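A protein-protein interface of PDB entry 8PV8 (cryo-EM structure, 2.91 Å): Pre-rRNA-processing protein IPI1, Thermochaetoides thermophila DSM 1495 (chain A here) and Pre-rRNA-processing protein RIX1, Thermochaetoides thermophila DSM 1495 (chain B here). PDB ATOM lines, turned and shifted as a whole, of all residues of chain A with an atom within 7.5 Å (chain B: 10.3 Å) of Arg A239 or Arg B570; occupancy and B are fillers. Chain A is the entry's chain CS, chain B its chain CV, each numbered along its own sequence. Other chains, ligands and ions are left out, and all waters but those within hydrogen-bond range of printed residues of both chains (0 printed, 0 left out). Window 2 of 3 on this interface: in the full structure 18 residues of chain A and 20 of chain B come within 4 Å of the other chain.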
ATOM      1  N   ASP A 171       4.273 -34.071   0.631  1.00  0.00           N
ATOM      2  CA  ASP A 171       3.948 -32.671   0.874  1.00  0.00           C
ATOM      3  C   ASP A 171       4.951 -31.708   0.259  1.00  0.00           C
ATOM      4  O   ASP A 171       4.543 -30.683  -0.299  1.00  0.00           O
ATOM      5  CB  ASP A 171       3.848 -32.407   2.378  1.00  0.00           C
ATOM      6  CG  ASP A 171       2.968 -33.416   3.086  1.00  0.00           C
ATOM      7  OD1 ASP A 171       2.059 -33.972   2.435  1.00  0.00           O
ATOM      8  OD2 ASP A 171       3.184 -33.654   4.292  1.00  0.00           O
ATOM      9  N   PHE A 233      -0.324 -39.063  -7.572  1.00  0.00           N
ATOM     10  CA  PHE A 233       0.082 -37.670  -7.408  1.00  0.00           C
ATOM     11  C   PHE A 233      -1.104 -36.780  -7.055  1.00  0.00           C
ATOM     12  O   PHE A 233      -1.003 -35.916  -6.175  1.00  0.00           O
ATOM     13  CB  PHE A 233       0.767 -37.185  -8.688  1.00  0.00           C
ATOM     14  CG  PHE A 233       1.239 -35.761  -8.630  1.00  0.00           C
ATOM     15  CD1 PHE A 233       2.387 -35.426  -7.931  1.00  0.00           C
ATOM     16  CD2 PHE A 233       0.551 -34.762  -9.301  1.00  0.00           C
ATOM     17  CE1 PHE A 233       2.830 -34.117  -7.884  1.00  0.00           C
ATOM     18  CE2 PHE A 233       0.990 -33.452  -9.260  1.00  0.00           C
ATOM     19  CZ  PHE A 233       2.130 -33.131  -8.551  1.00  0.00           C
ATOM     20  N   LEU A 234      -2.243 -36.988  -7.723  1.00  0.00           N
ATOM     21  CA  LEU A 234      -3.440 -36.209  -7.411  1.00  0.00           C
ATOM     22  C   LEU A 234      -3.977 -36.541  -6.023  1.00  0.00           C
ATOM     23  O   LEU A 234      -4.437 -35.647  -5.302  1.00  0.00           O
ATOM     24  CB  LEU A 234      -4.513 -36.440  -8.473  1.00  0.00           C
ATOM     25  CG  LEU A 234      -4.223 -35.843  -9.852  1.00  0.00           C
ATOM     26  CD1 LEU A 234      -5.405 -36.043 -10.785  1.00  0.00           C
ATOM     27  CD2 LEU A 234      -3.873 -34.369  -9.735  1.00  0.00           C
ATOM     28  N   GLN A 235      -3.929 -37.819  -5.633  1.00  0.00           N
ATOM     29  CA  GLN A 235      -4.347 -38.208  -4.289  1.00  0.00           C
ATOM     30  C   GLN A 235      -3.450 -37.586  -3.225  1.00  0.00           C
ATOM     31  O   GLN A 235      -3.934 -37.155  -2.173  1.00  0.00           O
ATOM     32  CB  GLN A 235      -4.348 -39.731  -4.160  1.00  0.00           C
ATOM     33  CG  GLN A 235      -5.635 -40.395  -4.616  1.00  0.00           C
ATOM     34  CD  GLN A 235      -6.794 -40.115  -3.682  1.00  0.00           C
ATOM     35  OE1 GLN A 235      -7.711 -39.366  -4.018  1.00  0.00           O
ATOM     36  NE2 GLN A 235      -6.758 -40.715  -2.499  1.00  0.00           N
ATOM     37  N   THR A 236      -2.141 -37.538  -3.481  1.00  0.00           N
ATOM     38  CA  THR A 236      -1.220 -36.895  -2.551  1.00  0.00           C
ATOM     39  C   THR A 236      -1.487 -35.396  -2.455  1.00  0.00           C
ATOM     40  O   THR A 236      -1.505 -34.831  -1.353  1.00  0.00           O
ATOM     41  CB  THR A 236       0.222 -37.158  -2.986  1.00  0.00           C
ATOM     42  OG1 THR A 236       0.475 -38.569  -2.964  1.00  0.00           O
ATOM     43  CG2 THR A 236       1.198 -36.467  -2.059  1.00  0.00           C
ATOM     44  N   GLY A 237      -1.718 -34.739  -3.595  1.00  0.00           N
ATOM     45  CA  GLY A 237      -2.004 -33.316  -3.584  1.00  0.00           C
ATOM     46  C   GLY A 237      -3.322 -32.940  -2.941  1.00  0.00           C
ATOM     47  O   GLY A 237      -3.420 -31.865  -2.340  1.00  0.00           O
ATOM     48  N   PHE A 238      -4.338 -33.797  -3.056  1.00  0.00           N
ATOM     49  CA  PHE A 238      -5.661 -33.538  -2.495  1.00  0.00           C
ATOM     50  C   PHE A 238      -5.970 -34.457  -1.318  1.00  0.00           C
ATOM     51  O   PHE A 238      -7.141 -34.752  -1.057  1.00  0.00           O
ATOM     52  CB  PHE A 238      -6.741 -33.675  -3.573  1.00  0.00           C
ATOM     53  CG  PHE A 238      -6.617 -32.694  -4.720  1.00  0.00           C
ATOM     54  CD1 PHE A 238      -5.830 -31.555  -4.627  1.00  0.00           C
ATOM     55  CD2 PHE A 238      -7.262 -32.947  -5.916  1.00  0.00           C
ATOM     56  CE1 PHE A 238      -5.724 -30.678  -5.685  1.00  0.00           C
ATOM     57  CE2 PHE A 238      -7.156 -32.077  -6.982  1.00  0.00           C
ATOM     58  CZ  PHE A 238      -6.384 -30.942  -6.866  1.00  0.00           C
ATOM     59  N   ARG A 239      -4.939 -34.929  -0.623  1.00  0.00           N
ATOM     60  CA  ARG A 239      -5.127 -35.796   0.531  1.00  0.00           C
ATOM     61  C   ARG A 239      -5.815 -35.025   1.658  1.00  0.00           C
ATOM     62  O   ARG A 239      -5.490 -33.857   1.898  1.00  0.00           O
ATOM     63  CB  ARG A 239      -3.765 -36.352   0.976  1.00  0.00           C
ATOM     64  CG  ARG A 239      -3.755 -37.436   2.061  1.00  0.00           C
ATOM     65  CD  ARG A 239      -3.654 -36.877   3.474  1.00  0.00           C
ATOM     66  NE  ARG A 239      -2.421 -36.126   3.676  1.00  0.00           N
ATOM     67  CZ  ARG A 239      -2.211 -35.285   4.681  1.00  0.00           C
ATOM     68  NH1 ARG A 239      -3.135 -35.062   5.600  1.00  0.00           N
ATOM     69  NH2 ARG A 239      -1.044 -34.653   4.763  1.00  0.00           N
ATOM     70  N   PRO A 240      -6.785 -35.639   2.341  1.00  0.00           N
ATOM     71  CA  PRO A 240      -7.517 -34.931   3.400  1.00  0.00           C
ATOM     72  C   PRO A 240      -6.621 -34.582   4.579  1.00  0.00           C
ATOM     73  O   PRO A 240      -5.980 -35.447   5.179  1.00  0.00           O
ATOM     74  CB  PRO A 240      -8.607 -35.930   3.805  1.00  0.00           C
ATOM     75  CG  PRO A 240      -8.785 -36.803   2.610  1.00  0.00           C
ATOM     76  CD  PRO A 240      -7.428 -36.915   1.980  1.00  0.00           C
ATOM     77  N   GLU A 241      -6.610 -33.300   4.928  1.00  0.00           N
ATOM     78  CA  GLU A 241      -5.667 -32.748   5.889  1.00  0.00           C
ATOM     79  C   GLU A 241      -6.327 -32.601   7.255  1.00  0.00           C
ATOM     80  O   GLU A 241      -7.474 -32.152   7.355  1.00  0.00           O
ATOM     81  CB  GLU A 241      -5.121 -31.408   5.384  1.00  0.00           C
ATOM     82  CG  GLU A 241      -6.180 -30.373   5.035  1.00  0.00           C
ATOM     83  CD  GLU A 241      -5.616 -29.212   4.245  1.00  0.00           C
ATOM     84  OE1 GLU A 241      -4.443 -29.295   3.826  1.00  0.00           O
ATOM     85  OE2 GLU A 241      -6.340 -28.213   4.055  1.00  0.00           O
ATOM     86  N   GLU A 242      -5.608 -33.016   8.302  1.00  0.00           N
ATOM     87  CA  GLU A 242      -6.043 -32.950   9.687  1.00  0.00           C
ATOM     88  C   GLU A 242      -5.063 -32.114  10.503  1.00  0.00           C
ATOM     89  O   GLU A 242      -3.853 -32.364  10.458  1.00  0.00           O
ATOM     90  CB  GLU A 242      -6.153 -34.358  10.288  1.00  0.00           C
ATOM     91  CG  GLU A 242      -6.920 -34.449  11.602  1.00  0.00           C
ATOM     92  CD  GLU A 242      -6.036 -34.272  12.819  1.00  0.00           C
ATOM     93  OE1 GLU A 242      -4.845 -34.644  12.748  1.00  0.00           O
ATOM     94  OE2 GLU A 242      -6.532 -33.766  13.847  1.00  0.00           O
ATOM     95  N   PRO A 243      -5.547 -31.116  11.244  1.00  0.00           N
ATOM     96  CA  PRO A 243      -4.632 -30.191  11.923  1.00  0.00           C
ATOM     97  C   PRO A 243      -3.921 -30.824  13.110  1.00  0.00           C
ATOM     98  O   PRO A 243      -4.412 -31.767  13.736  1.00  0.00           O
ATOM     99  CB  PRO A 243      -5.556 -29.055  12.380  1.00  0.00           C
ATOM    100  CG  PRO A 243      -6.898 -29.691  12.497  1.00  0.00           C
ATOM    101  CD  PRO A 243      -6.957 -30.732  11.416  1.00  0.00           C
ATOM    102  N   LEU A 244      -2.750 -30.283  13.412  1.00  0.00           N
ATOM    103  CA  LEU A 244      -1.954 -30.681  14.564  1.00  0.00           C
ATOM    104  C   LEU A 244      -2.584 -30.125  15.833  1.00  0.00           C
ATOM    105  O   LEU A 244      -3.131 -29.020  15.837  1.00  0.00           O
ATOM    106  CB  LEU A 244      -0.524 -30.168  14.387  1.00  0.00           C
ATOM    107  CG  LEU A 244       0.627 -30.443  15.361  1.00  0.00           C
ATOM    108  CD1 LEU A 244       0.954 -31.929  15.449  1.00  0.00           C
ATOM    109  CD2 LEU A 244       1.863 -29.648  14.962  1.00  0.00           C
ATOM    110  N   PRO A 245      -2.541 -30.877  16.947  1.00  0.00           N
ATOM    111  CA  PRO A 245      -3.084 -30.350  18.210  1.00  0.00           C
ATOM    112  C   PRO A 245      -2.295 -29.181  18.783  1.00  0.00           C
ATOM    113  O   PRO A 245      -1.249 -28.795  18.251  1.00  0.00           O
ATOM    114  CB  PRO A 245      -3.041 -31.566  19.145  1.00  0.00           C
ATOM    115  CG  PRO A 245      -2.052 -32.496  18.527  1.00  0.00           C
ATOM    116  CD  PRO A 245      -2.227 -32.311  17.054  1.00  0.00           C
ATOM    117  N   PRO A 283       0.832 -24.303  -1.360  1.00  0.00           N
ATOM    118  CA  PRO A 283       0.998 -25.198  -0.206  1.00  0.00           C
ATOM    119  C   PRO A 283      -0.291 -25.867   0.246  1.00  0.00           C
ATOM    120  O   PRO A 283      -0.272 -27.026   0.670  1.00  0.00           O
ATOM    121  CB  PRO A 283       1.548 -24.266   0.882  1.00  0.00           C
ATOM    122  CG  PRO A 283       1.102 -22.904   0.485  1.00  0.00           C
ATOM    123  CD  PRO A 283       1.037 -22.887  -1.011  1.00  0.00           C
ATOM    124  N   ASP A 284      -1.411 -25.156   0.165  1.00  0.00           N
ATOM    125  CA  ASP A 284      -2.650 -25.690   0.710  1.00  0.00           C
ATOM    126  C   ASP A 284      -3.546 -26.282  -0.376  1.00  0.00           C
ATOM    127  O   ASP A 284      -3.487 -25.908  -1.558  1.00  0.00           O
ATOM    128  CB  ASP A 284      -3.395 -24.611   1.503  1.00  0.00           C
ATOM    129  CG  ASP A 284      -3.651 -23.355   0.697  1.00  0.00           C
ATOM    130  OD1 ASP A 284      -3.160 -23.259  -0.444  1.00  0.00           O
ATOM    131  OD2 ASP A 284      -4.353 -22.458   1.208  1.00  0.00           O
ATOM    132  N   ARG A 285      -4.393 -27.224   0.054  1.00  0.00           N
ATOM    133  CA  ARG A 285      -5.265 -27.929  -0.876  1.00  0.00           C
ATOM    134  C   ARG A 285      -6.324 -27.012  -1.467  1.00  0.00           C
ATOM    135  O   ARG A 285      -6.864 -27.316  -2.532  1.00  0.00           O
ATOM    136  CB  ARG A 285      -5.934 -29.123  -0.193  1.00  0.00           C
ATOM    137  CG  ARG A 285      -6.958 -28.749   0.862  1.00  0.00           C
ATOM    138  CD  ARG A 285      -7.695 -29.972   1.371  1.00  0.00           C
ATOM    139  NE  ARG A 285      -8.575 -30.522   0.346  1.00  0.00           N
ATOM    140  CZ  ARG A 285      -9.116 -31.732   0.389  1.00  0.00           C
ATOM    141  NH1 ARG A 285      -8.892 -32.553   1.401  1.00  0.00           N
ATOM    142  NH2 ARG A 285      -9.903 -32.126  -0.608  1.00  0.00           N
ATOM    143  N   ARG A 288      -4.481 -25.539  -4.389  1.00  0.00           N
ATOM    144  CA  ARG A 288      -4.241 -26.649  -5.312  1.00  0.00           C
ATOM    145  C   ARG A 288      -5.515 -27.040  -6.057  1.00  0.00           C
ATOM    146  O   ARG A 288      -5.505 -27.211  -7.283  1.00  0.00           O
ATOM    147  CB  ARG A 288      -3.671 -27.847  -4.556  1.00  0.00           C
ATOM    148  CG  ARG A 288      -2.155 -27.956  -4.599  1.00  0.00           C
ATOM    149  CD  ARG A 288      -1.664 -29.033  -3.650  1.00  0.00           C
ATOM    150  NE  ARG A 288      -1.788 -28.630  -2.254  1.00  0.00           N
ATOM    151  CZ  ARG A 288      -1.626 -29.446  -1.222  1.00  0.00           C
ATOM    152  NH1 ARG A 288      -1.376 -30.733  -1.392  1.00  0.00           N
ATOM    153  NH2 ARG A 288      -1.727 -28.960   0.011  1.00  0.00           N
ATOM    154  N   TYR B 566       1.178 -16.665  10.826  1.00  0.00           N
ATOM    155  CA  TYR B 566       0.205 -17.318   9.959  1.00  0.00           C
ATOM    156  C   TYR B 566       0.346 -18.830  10.100  1.00  0.00           C
ATOM    157  O   TYR B 566       1.419 -19.385   9.844  1.00  0.00           O
ATOM    158  CB  TYR B 566       0.406 -16.872   8.512  1.00  0.00           C
ATOM    159  CG  TYR B 566      -0.524 -17.521   7.514  1.00  0.00           C
ATOM    160  CD1 TYR B 566      -1.816 -17.048   7.331  1.00  0.00           C
ATOM    161  CD2 TYR B 566      -0.102 -18.590   6.736  1.00  0.00           C
ATOM    162  CE1 TYR B 566      -2.667 -17.636   6.414  1.00  0.00           C
ATOM    163  CE2 TYR B 566      -0.946 -19.183   5.817  1.00  0.00           C
ATOM    164  CZ  TYR B 566      -2.226 -18.701   5.660  1.00  0.00           C
ATOM    165  OH  TYR B 566      -3.069 -19.288   4.745  1.00  0.00           O
ATOM    166  N   ARG B 567      -0.733 -19.490  10.510  1.00  0.00           N
ATOM    167  CA  ARG B 567      -0.778 -20.945  10.552  1.00  0.00           C
ATOM    168  C   ARG B 567      -1.060 -21.501   9.165  1.00  0.00           C
ATOM    169  O   ARG B 567      -1.846 -20.934   8.402  1.00  0.00           O
ATOM    170  CB  ARG B 567      -1.851 -21.436  11.523  1.00  0.00           C
ATOM    171  CG  ARG B 567      -1.585 -21.142  12.981  1.00  0.00           C
ATOM    172  CD  ARG B 567      -2.711 -21.716  13.814  1.00  0.00           C
ATOM    173  NE  ARG B 567      -2.588 -21.408  15.232  1.00  0.00           N
ATOM    174  CZ  ARG B 567      -1.930 -22.152  16.108  1.00  0.00           C
ATOM    175  NH1 ARG B 567      -1.285 -23.248  15.741  1.00  0.00           N
ATOM    176  NH2 ARG B 567      -1.911 -21.787  17.386  1.00  0.00           N
ATOM    177  N   ASP B 568      -0.412 -22.616   8.842  1.00  0.00           N
ATOM    178  CA  ASP B 568      -0.685 -23.309   7.592  1.00  0.00           C
ATOM    179  C   ASP B 568      -1.896 -24.224   7.780  1.00  0.00           C
ATOM    180  O   ASP B 568      -2.619 -24.144   8.777  1.00  0.00           O
ATOM    181  CB  ASP B 568       0.559 -24.056   7.109  1.00  0.00           C
ATOM    182  CG  ASP B 568       1.135 -25.006   8.154  1.00  0.00           C
ATOM    183  OD1 ASP B 568       0.519 -25.208   9.221  1.00  0.00           O
ATOM    184  OD2 ASP B 568       2.225 -25.557   7.899  1.00  0.00           O
ATOM    185  N   SER B 569      -2.135 -25.104   6.807  1.00  0.00           N
ATOM    186  CA  SER B 569      -3.199 -26.088   6.956  1.00  0.00           C
ATOM    187  C   SER B 569      -2.836 -27.135   8.003  1.00  0.00           C
ATOM    188  O   SER B 569      -3.719 -27.707   8.651  1.00  0.00           O
ATOM    189  CB  SER B 569      -3.492 -26.745   5.609  1.00  0.00           C
ATOM    190  OG  SER B 569      -2.325 -27.336   5.063  1.00  0.00           O
ATOM    191  N   ARG B 570      -1.537 -27.392   8.181  1.00  0.00           N
ATOM    192  CA  ARG B 570      -1.051 -28.330   9.186  1.00  0.00           C
ATOM    193  C   ARG B 570      -1.167 -27.790  10.603  1.00  0.00           C
ATOM    194  O   ARG B 570      -1.033 -28.564  11.556  1.00  0.00           O
ATOM    195  CB  ARG B 570       0.411 -28.697   8.902  1.00  0.00           C
ATOM    196  CG  ARG B 570       0.681 -29.255   7.507  1.00  0.00           C
ATOM    197  CD  ARG B 570       0.679 -30.788   7.487  1.00  0.00           C
ATOM    198  NE  ARG B 570      -0.573 -31.384   7.942  1.00  0.00           N
ATOM    199  CZ  ARG B 570      -1.704 -31.390   7.248  1.00  0.00           C
ATOM    200  NH1 ARG B 570      -1.780 -30.861   6.038  1.00  0.00           N
ATOM    201  NH2 ARG B 570      -2.786 -31.953   7.780  1.00  0.00           N
ATOM    202  N   GLY B 571      -1.415 -26.495  10.766  1.00  0.00           N
ATOM    203  CA  GLY B 571      -1.420 -25.872  12.070  1.00  0.00           C
ATOM    204  C   GLY B 571      -0.079 -25.344  12.522  1.00  0.00           C
ATOM    205  O   GLY B 571      -0.010 -24.707  13.578  1.00  0.00           O
ATOM    206  N   ARG B 572       0.982 -25.584  11.759  1.00  0.00           N
ATOM    207  CA  ARG B 572       2.306 -25.070  12.077  1.00  0.00           C
ATOM    208  C   ARG B 572       2.418 -23.604  11.681  1.00  0.00           C
ATOM    209  O   ARG B 572       1.853 -23.174  10.673  1.00  0.00           O
ATOM    210  CB  ARG B 572       3.379 -25.884  11.354  1.00  0.00           C
ATOM    211  CG  ARG B 572       3.512 -27.314  11.858  1.00  0.00           C
ATOM    212  CD  ARG B 572       4.640 -28.052  11.151  1.00  0.00           C
ATOM    213  NE  ARG B 572       4.329 -28.306   9.750  1.00  0.00           N
ATOM    214  CZ  ARG B 572       4.964 -27.745   8.731  1.00  0.00           C
ATOM    215  NH1 ARG B 572       5.953 -26.886   8.920  1.00  0.00           N
ATOM    216  NH2 ARG B 572       4.593 -28.045   7.489  1.00  0.00           N
ATOM    217  N   TYR B 573       3.165 -22.842  12.469  1.00  0.00           N
ATOM    218  CA  TYR B 573       3.355 -21.437  12.161  1.00  0.00           C
ATOM    219  C   TYR B 573       4.383 -21.247  11.048  1.00  0.00           C
ATOM    220  O   TYR B 573       5.341 -22.011  10.903  1.00  0.00           O
ATOM    221  CB  TYR B 573       3.801 -20.670  13.401  1.00  0.00           C
ATOM    222  CG  TYR B 573       2.840 -20.707  14.570  1.00  0.00           C
ATOM    223  CD1 TYR B 573       2.904 -21.712  15.524  1.00  0.00           C
ATOM    224  CD2 TYR B 573       1.874 -19.726  14.720  1.00  0.00           C
ATOM    225  CE1 TYR B 573       2.036 -21.730  16.593  1.00  0.00           C
ATOM    226  CE2 TYR B 573       1.002 -19.738  15.785  1.00  0.00           C
ATOM    227  CZ  TYR B 573       1.099 -20.738  16.722  1.00  0.00           C
ATOM    228  OH  TYR B 573       0.239 -20.768  17.789  1.00  0.00           O
ATOM    229  N   TYR B 574       4.168 -20.206  10.256  1.00  0.00           N
ATOM    230  CA  TYR B 574       5.149 -19.772   9.280  1.00  0.00           C
ATOM    231  C   TYR B 574       6.360 -19.177   9.991  1.00  0.00           C
ATOM    232  O   TYR B 574       6.249 -18.697  11.122  1.00  0.00           O
ATOM    233  CB  TYR B 574       4.527 -18.741   8.342  1.00  0.00           C
ATOM    234  CG  TYR B 574       3.855 -19.329   7.123  1.00  0.00           C
ATOM    235  CD1 TYR B 574       3.182 -20.543   7.187  1.00  0.00           C
ATOM    236  CD2 TYR B 574       3.874 -18.657   5.910  1.00  0.00           C
ATOM    237  CE1 TYR B 574       2.561 -21.080   6.069  1.00  0.00           C
ATOM    238  CE2 TYR B 574       3.255 -19.183   4.787  1.00  0.00           C
ATOM    239  CZ  TYR B 574       2.599 -20.395   4.872  1.00  0.00           C
ATOM    240  OH  TYR B 574       1.980 -20.928   3.763  1.00  0.00           O
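The side-chain hydroxyl of Ser B569 is in hydrogen-bond range of the side-chain carboxylate of Glu A241.
The guanidinium group (NH2) of Arg B570 sits at hydrogen-bond distance from the backbone carbonyl oxygen (O) of Glu A242, 2.9 Å away.
N of Leu A244 sits at hydrogen-bond distance from O of Arg B570.
OE1 of Glu A241 is in salt-bridge range of NH1 of Arg B570 (3.8 Å).
The backbone carbonyl oxygen (O) of Pro A283 sits at hydrogen-bond distance from the guanidinium group (NH2) of Arg A288 (2.5 Å).
The side-chain carboxylate (OD1) of Asp B568 lies within hydrogen-bond range of the backbone NH (N) of Arg B570 (3.2 Å).
OD1 of Asp A171 lies within salt-bridge range of NH2 of Arg A239 (3.9 Å).
The backbone NH (N) of Tyr B574 sits at hydrogen-bond distance from the backbone carbonyl oxygen (O) of Tyr B566 (2.9 Å).
Among the printed residues, merely in contact across the chains: Arg A239 with Arg B570, Pro A283 with Tyr B574 and Pro A243 with Arg B570.
No residue of chain B comes within 4 Å of Gly A237.
No residue of chain B comes within 4 Å of Pro A240.
Of chain B, only Ser B569 and Arg B570 come within 4 Å of Glu A241.
Pro A243 touches one residue of chain B.
Leu A244 touches one residue of chain B.
Of the printed residues of chain A, Ser B569 touches Glu A241.
Of the printed residues of chain A, Tyr B574 touches Pro A283 (3.9 Å).
Of the printed residues of chain B, Pro A283 touches Tyr B574 (3.9 Å).
The nearest residue of chain B that does not touch Arg A239 is Ser B569 (7.4 Å).
The nearest printed residue of chain B that does not touch Pro A283 is Ser B569 (4.9 Å).
Of the 9 printed residues of chain B, 3 touch a printed residue of chain A.
Printed residues of chain B that touch a printed residue of chain A: Ser B569, Arg B570 and Tyr B574.
Along chain B the printed residues that touch a printed residue of chain A span positions 569 to 574.
Along chain A the printed residues that touch a printed residue of chain B span positions 239 to 283.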
